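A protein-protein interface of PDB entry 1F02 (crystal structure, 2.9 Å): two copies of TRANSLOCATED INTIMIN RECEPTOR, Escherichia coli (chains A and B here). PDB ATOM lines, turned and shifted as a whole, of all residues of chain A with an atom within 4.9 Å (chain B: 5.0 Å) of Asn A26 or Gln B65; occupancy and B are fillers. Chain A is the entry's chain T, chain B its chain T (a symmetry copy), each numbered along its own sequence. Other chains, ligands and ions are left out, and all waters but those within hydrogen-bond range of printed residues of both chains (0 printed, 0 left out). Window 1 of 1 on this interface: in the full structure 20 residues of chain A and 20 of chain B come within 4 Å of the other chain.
No position is printed for both chains. Of the 8 pairs that touch across the chains among the printed residues, none has its exchanged pair printed and touching as well.
O of Ala A20 sits close to OD1 of Asn A26. OE1 of Gln B65 sits close to O of Val B61, at 2.8 Å. The side-chain amide nitrogen of Asn A23 lies close to the backbone NH of Glu A25 (2.9 Å). The backbone carbonyl oxygen of Asn A26 sits at hydrogen-bond distance from the backbone NH of Lys A44 (2.7 Å).
OD1 of Asn A26 lies close to O of Gln B65, at 2.8 Å. The backbone carbonyl oxygen of Gln B65 lies close to the side-chain amide oxygen of Asn A23 (3.3 Å). The backbone carbonyl oxygen of Ile A47 lies close to the side-chain amide nitrogen of Gln B65 (3.5 Å).
Of the printed residues of chain B, Asn A26 touches Gln B65 (2.8 Å). Of the printed residues of chain A, Val B61 touches Gln A50. Gln B65 touches just these residues of chain A: Asn A23 (3.3 Å), Asn A26 (2.8 Å), Ile A47 (3.0 Å), Gln A50 (3.6 Å) and Ile A51 (3.9 Å). Of the printed residues of chain A, Ala B66 touches Asn A23 (3.9 Å). The nearest residue of chain A that does not touch Gln B65 is Leu A16 (4.6 Å).
Among the printed residues, merely in contact across the chains: Leu A16 with Ala B62, Asn A23 with Ala B66, Gln A50 with Val B61, Gln A50 with Gln B65 and Ile A51 with Gln B65.
Printed residues of chain B that touch a printed residue of chain A: Val B61, Ala B62, Gln B65 and Ala B66. Hydrophobic or aromatic side chains of chain B that line the printed part of chain A: Val B61. Along chain B the printed residues that touch a printed residue of chain A span positions 61 to 66. Printed residues of chain A that touch a printed residue of chain B: Leu A16, Asn A23, Asn A26, Ile A47, Gln A50 and Ile A51. Hydrophobic or aromatic side chains of chain A within 4 Å of the printed part of chain B: Leu A16, Ile A47 and Ile A51. Among the printed residues, no Asp or Glu carboxylate lies within 4 Å of a Lys or Arg side-chain nitrogen of the other chain.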
ATOM      1  N   LEU A  16      12.201   8.137  -5.363  1.00  0.00           N
ATOM      2  CA  LEU A  16      11.514   8.200  -4.080  1.00  0.00           C
ATOM      3  C   LEU A  16      11.120   9.644  -3.820  1.00  0.00           C
ATOM      4  O   LEU A  16      10.068   9.911  -3.249  1.00  0.00           O
ATOM      5  CB  LEU A  16      12.408   7.691  -2.949  1.00  0.00           C
ATOM      6  CG  LEU A  16      12.370   6.175  -2.717  1.00  0.00           C
ATOM      7  CD1 LEU A  16      13.285   5.832  -1.554  1.00  0.00           C
ATOM      8  CD2 LEU A  16      10.952   5.717  -2.415  1.00  0.00           C
ATOM      9  N   ALA A  20       7.258  11.391  -3.339  1.00  0.00           N
ATOM     10  CA  ALA A  20       6.995  12.069  -2.079  1.00  0.00           C
ATOM     11  C   ALA A  20       6.066  13.277  -2.250  1.00  0.00           C
ATOM     12  O   ALA A  20       5.166  13.499  -1.435  1.00  0.00           O
ATOM     13  CB  ALA A  20       8.313  12.505  -1.443  1.00  0.00           C
ATOM     14  N   ASN A  23       2.097  13.646  -2.478  1.00  0.00           N
ATOM     15  CA  ASN A  23       1.414  13.648  -1.190  1.00  0.00           C
ATOM     16  C   ASN A  23       1.838  14.896  -0.397  1.00  0.00           C
ATOM     17  O   ASN A  23       2.996  15.021   0.027  1.00  0.00           O
ATOM     18  CB  ASN A  23       1.770  12.391  -0.401  1.00  0.00           C
ATOM     19  CG  ASN A  23       1.181  12.401   0.989  1.00  0.00           C
ATOM     20  OD1 ASN A  23       1.436  11.503   1.792  1.00  0.00           O
ATOM     21  ND2 ASN A  23       0.381  13.424   1.284  1.00  0.00           N
ATOM     22  N   PRO A  24       0.892  15.827  -0.178  1.00  0.00           N
ATOM     23  CA  PRO A  24       1.100  17.087   0.548  1.00  0.00           C
ATOM     24  C   PRO A  24       1.650  16.895   1.951  1.00  0.00           C
ATOM     25  O   PRO A  24       2.454  17.690   2.422  1.00  0.00           O
ATOM     26  CB  PRO A  24      -0.290  17.706   0.562  1.00  0.00           C
ATOM     27  CG  PRO A  24      -0.906  17.173  -0.688  1.00  0.00           C
ATOM     28  CD  PRO A  24      -0.503  15.727  -0.635  1.00  0.00           C
ATOM     29  N   GLU A  25       1.197  15.834   2.608  1.00  0.00           N
ATOM     30  CA  GLU A  25       1.626  15.499   3.964  1.00  0.00           C
ATOM     31  C   GLU A  25       3.125  15.717   4.172  1.00  0.00           C
ATOM     32  O   GLU A  25       3.556  16.506   5.022  1.00  0.00           O
ATOM     33  CB  GLU A  25       1.308  14.026   4.249  1.00  0.00           C
ATOM     34  CG  GLU A  25      -0.155  13.649   4.107  1.00  0.00           C
ATOM     35  CD  GLU A  25      -0.980  14.068   5.303  1.00  0.00           C
ATOM     36  OE1 GLU A  25      -0.845  15.235   5.743  1.00  0.00           O
ATOM     37  OE2 GLU A  25      -1.767  13.228   5.797  1.00  0.00           O
ATOM     38  N   ASN A  26       3.897  14.991   3.373  1.00  0.00           N
ATOM     39  CA  ASN A  26       5.353  14.999   3.407  1.00  0.00           C
ATOM     40  C   ASN A  26       5.996  16.359   3.184  1.00  0.00           C
ATOM     41  O   ASN A  26       7.128  16.585   3.608  1.00  0.00           O
ATOM     42  CB  ASN A  26       5.869  14.033   2.347  1.00  0.00           C
ATOM     43  CG  ASN A  26       5.060  12.755   2.285  1.00  0.00           C
ATOM     44  OD1 ASN A  26       5.005  12.092   1.247  1.00  0.00           O
ATOM     45  ND2 ASN A  26       4.432  12.397   3.401  1.00  0.00           N
ATOM     46  N   GLN A  27       5.286  17.263   2.522  1.00  0.00           N
ATOM     47  CA  GLN A  27       5.849  18.574   2.233  1.00  0.00           C
ATOM     48  C   GLN A  27       5.886  19.545   3.394  1.00  0.00           C
ATOM     49  O   GLN A  27       5.325  19.298   4.459  1.00  0.00           O
ATOM     50  CB  GLN A  27       5.096  19.222   1.084  1.00  0.00           C
ATOM     51  CG  GLN A  27       4.849  18.278  -0.053  1.00  0.00           C
ATOM     52  CD  GLN A  27       4.473  19.003  -1.313  1.00  0.00           C
ATOM     53  OE1 GLN A  27       4.024  18.386  -2.274  1.00  0.00           O
ATOM     54  NE2 GLN A  27       4.663  20.325  -1.323  1.00  0.00           N
ATOM     55  N   LYS A  28       6.577  20.653   3.167  1.00  0.00           N
ATOM     56  CA  LYS A  28       6.701  21.710   4.154  1.00  0.00           C
ATOM     57  C   LYS A  28       5.946  22.899   3.584  1.00  0.00           C
ATOM     58  O   LYS A  28       5.541  22.881   2.414  1.00  0.00           O
ATOM     59  CB  LYS A  28       8.170  22.087   4.363  1.00  0.00           C
ATOM     60  CG  LYS A  28       9.004  21.062   5.115  1.00  0.00           C
ATOM     61  CD  LYS A  28      10.426  21.590   5.309  1.00  0.00           C
ATOM     62  CE  LYS A  28      11.265  20.738   6.258  1.00  0.00           C
ATOM     63  NZ  LYS A  28      12.606  21.351   6.510  1.00  0.00           N
ATOM     64  N   LEU A  43      10.911  19.034   1.292  1.00  0.00           N
ATOM     65  CA  LEU A  43      10.129  17.987   1.947  1.00  0.00           C
ATOM     66  C   LEU A  43      10.501  17.949   3.431  1.00  0.00           C
ATOM     67  O   LEU A  43      11.516  18.522   3.832  1.00  0.00           O
ATOM     68  CB  LEU A  43      10.440  16.620   1.336  1.00  0.00           C
ATOM     69  CG  LEU A  43      10.036  16.285  -0.099  1.00  0.00           C
ATOM     70  CD1 LEU A  43      10.530  14.891  -0.430  1.00  0.00           C
ATOM     71  CD2 LEU A  43       8.525  16.337  -0.258  1.00  0.00           C
ATOM     72  N   LYS A  44       9.682  17.272   4.240  1.00  0.00           N
ATOM     73  CA  LYS A  44       9.951  17.139   5.678  1.00  0.00           C
ATOM     74  C   LYS A  44      11.262  16.377   5.901  1.00  0.00           C
ATOM     75  O   LYS A  44      11.543  15.385   5.212  1.00  0.00           O
ATOM     76  CB  LYS A  44       8.825  16.375   6.386  1.00  0.00           C
ATOM     77  CG  LYS A  44       7.556  17.157   6.663  1.00  0.00           C
ATOM     78  CD  LYS A  44       6.549  16.237   7.325  1.00  0.00           C
ATOM     79  CE  LYS A  44       5.199  16.886   7.478  1.00  0.00           C
ATOM     80  NZ  LYS A  44       4.165  15.841   7.742  1.00  0.00           N
ATOM     81  N   ASP A  46      12.369  14.206   8.217  1.00  0.00           N
ATOM     82  CA  ASP A  46      12.306  12.762   8.431  1.00  0.00           C
ATOM     83  C   ASP A  46      11.978  12.027   7.128  1.00  0.00           C
ATOM     84  O   ASP A  46      12.016  10.796   7.074  1.00  0.00           O
ATOM     85  CB  ASP A  46      11.278  12.398   9.515  1.00  0.00           C
ATOM     86  CG  ASP A  46       9.850  12.647   9.080  1.00  0.00           C
ATOM     87  OD1 ASP A  46       8.930  12.099   9.728  1.00  0.00           O
ATOM     88  OD2 ASP A  46       9.649  13.393   8.099  1.00  0.00           O
ATOM     89  N   ILE A  47      11.657  12.785   6.084  1.00  0.00           N
ATOM     90  CA  ILE A  47      11.348  12.200   4.782  1.00  0.00           C
ATOM     91  C   ILE A  47      12.594  12.251   3.906  1.00  0.00           C
ATOM     92  O   ILE A  47      12.919  11.285   3.213  1.00  0.00           O
ATOM     93  CB  ILE A  47      10.194  12.955   4.081  1.00  0.00           C
ATOM     94  CG1 ILE A  47       8.880  12.697   4.827  1.00  0.00           C
ATOM     95  CG2 ILE A  47      10.087  12.521   2.615  1.00  0.00           C
ATOM     96  CD1 ILE A  47       8.459  11.232   4.881  1.00  0.00           C
ATOM     97  N   GLN A  50      14.809   9.745   5.455  1.00  0.00           N
ATOM     98  CA  GLN A  50      14.314   8.426   5.073  1.00  0.00           C
ATOM     99  C   GLN A  50      14.544   8.050   3.600  1.00  0.00           C
ATOM    100  O   GLN A  50      14.528   6.866   3.257  1.00  0.00           O
ATOM    101  CB  GLN A  50      12.821   8.337   5.417  1.00  0.00           C
ATOM    102  CG  GLN A  50      12.265   6.922   5.553  1.00  0.00           C
ATOM    103  CD  GLN A  50      10.803   6.912   5.990  1.00  0.00           C
ATOM    104  OE1 GLN A  50      10.439   7.515   7.006  1.00  0.00           O
ATOM    105  NE2 GLN A  50       9.960   6.224   5.224  1.00  0.00           N
ATOM    106  N   ILE A  51      14.733   9.039   2.725  1.00  0.00           N
ATOM    107  CA  ILE A  51      14.989   8.733   1.316  1.00  0.00           C
ATOM    108  C   ILE A  51      16.502   8.629   1.130  1.00  0.00           C
ATOM    109  O   ILE A  51      17.000   7.640   0.588  1.00  0.00           O
ATOM    110  CB  ILE A  51      14.426   9.817   0.328  1.00  0.00           C
ATOM    111  CG1 ILE A  51      15.103  11.174   0.569  1.00  0.00           C
ATOM    112  CG2 ILE A  51      12.908   9.916   0.464  1.00  0.00           C
ATOM    113  CD1 ILE A  51      14.758  12.238  -0.455  1.00  0.00           C
ATOM    114  N   VAL B  61       9.605   1.981   1.168  1.00  0.00           N
ATOM    115  CA  VAL B  61       9.708   3.314   1.725  1.00  0.00           C
ATOM    116  C   VAL B  61       8.862   4.228   0.846  1.00  0.00           C
ATOM    117  O   VAL B  61       8.723   5.419   1.115  1.00  0.00           O
ATOM    118  CB  VAL B  61      11.162   3.787   1.721  1.00  0.00           C
ATOM    119  CG1 VAL B  61      11.277   5.188   2.322  1.00  0.00           C
ATOM    120  CG2 VAL B  61      12.001   2.800   2.502  1.00  0.00           C
ATOM    121  N   ALA B  62       8.299   3.655  -0.213  1.00  0.00           N
ATOM    122  CA  ALA B  62       7.446   4.399  -1.134  1.00  0.00           C
ATOM    123  C   ALA B  62       6.055   4.517  -0.527  1.00  0.00           C
ATOM    124  O   ALA B  62       5.640   5.605  -0.121  1.00  0.00           O
ATOM    125  CB  ALA B  62       7.366   3.684  -2.472  1.00  0.00           C
ATOM    126  N   ARG B  63       5.345   3.392  -0.456  1.00  0.00           N
ATOM    127  CA  ARG B  63       3.993   3.370   0.097  1.00  0.00           C
ATOM    128  C   ARG B  63       3.948   3.964   1.507  1.00  0.00           C
ATOM    129  O   ARG B  63       3.090   4.788   1.809  1.00  0.00           O
ATOM    130  CB  ARG B  63       3.437   1.938   0.126  1.00  0.00           C
ATOM    131  CG  ARG B  63       4.071   1.045   1.179  1.00  0.00           C
ATOM    132  CD  ARG B  63       3.352  -0.294   1.340  1.00  0.00           C
ATOM    133  NE  ARG B  63       3.658  -1.259   0.283  1.00  0.00           N
ATOM    134  CZ  ARG B  63       3.095  -1.274  -0.923  1.00  0.00           C
ATOM    135  NH1 ARG B  63       2.177  -0.371  -1.245  1.00  0.00           N
ATOM    136  NH2 ARG B  63       3.449  -2.198  -1.810  1.00  0.00           N
ATOM    137  N   GLN B  64       4.875   3.554   2.367  1.00  0.00           N
ATOM    138  CA  GLN B  64       4.910   4.056   3.732  1.00  0.00           C
ATOM    139  C   GLN B  64       4.885   5.586   3.809  1.00  0.00           C
ATOM    140  O   GLN B  64       4.444   6.148   4.816  1.00  0.00           O
ATOM    141  CB  GLN B  64       6.139   3.499   4.467  1.00  0.00           C
ATOM    142  CG  GLN B  64       6.043   1.998   4.790  1.00  0.00           C
ATOM    143  CD  GLN B  64       7.352   1.399   5.310  1.00  0.00           C
ATOM    144  OE1 GLN B  64       7.402   0.229   5.696  1.00  0.00           O
ATOM    145  NE2 GLN B  64       8.415   2.201   5.315  1.00  0.00           N
ATOM    146  N   GLN B  65       5.350   6.265   2.758  1.00  0.00           N
ATOM    147  CA  GLN B  65       5.344   7.734   2.745  1.00  0.00           C
ATOM    148  C   GLN B  65       4.157   8.298   1.953  1.00  0.00           C
ATOM    149  O   GLN B  65       4.076   9.506   1.721  1.00  0.00           O
ATOM    150  CB  GLN B  65       6.647   8.286   2.150  1.00  0.00           C
ATOM    151  CG  GLN B  65       7.872   8.195   3.046  1.00  0.00           C
ATOM    152  CD  GLN B  65       9.145   8.625   2.325  1.00  0.00           C
ATOM    153  OE1 GLN B  65       9.417   8.178   1.209  1.00  0.00           O
ATOM    154  NE2 GLN B  65       9.934   9.484   2.962  1.00  0.00           N
ATOM    155  N   ALA B  66       3.241   7.423   1.547  1.00  0.00           N
ATOM    156  CA  ALA B  66       2.068   7.831   0.779  1.00  0.00           C
ATOM    157  C   ALA B  66       0.737   7.485   1.466  1.00  0.00           C
ATOM    158  O   ALA B  66       0.720   7.227   2.699  1.00  0.00           O
ATOM    159  CB  ALA B  66       2.116   7.201  -0.617  1.00  0.00           C
ATOM    160  OXT ALA B  66      -0.287   7.497   0.743  1.00  0.00           O
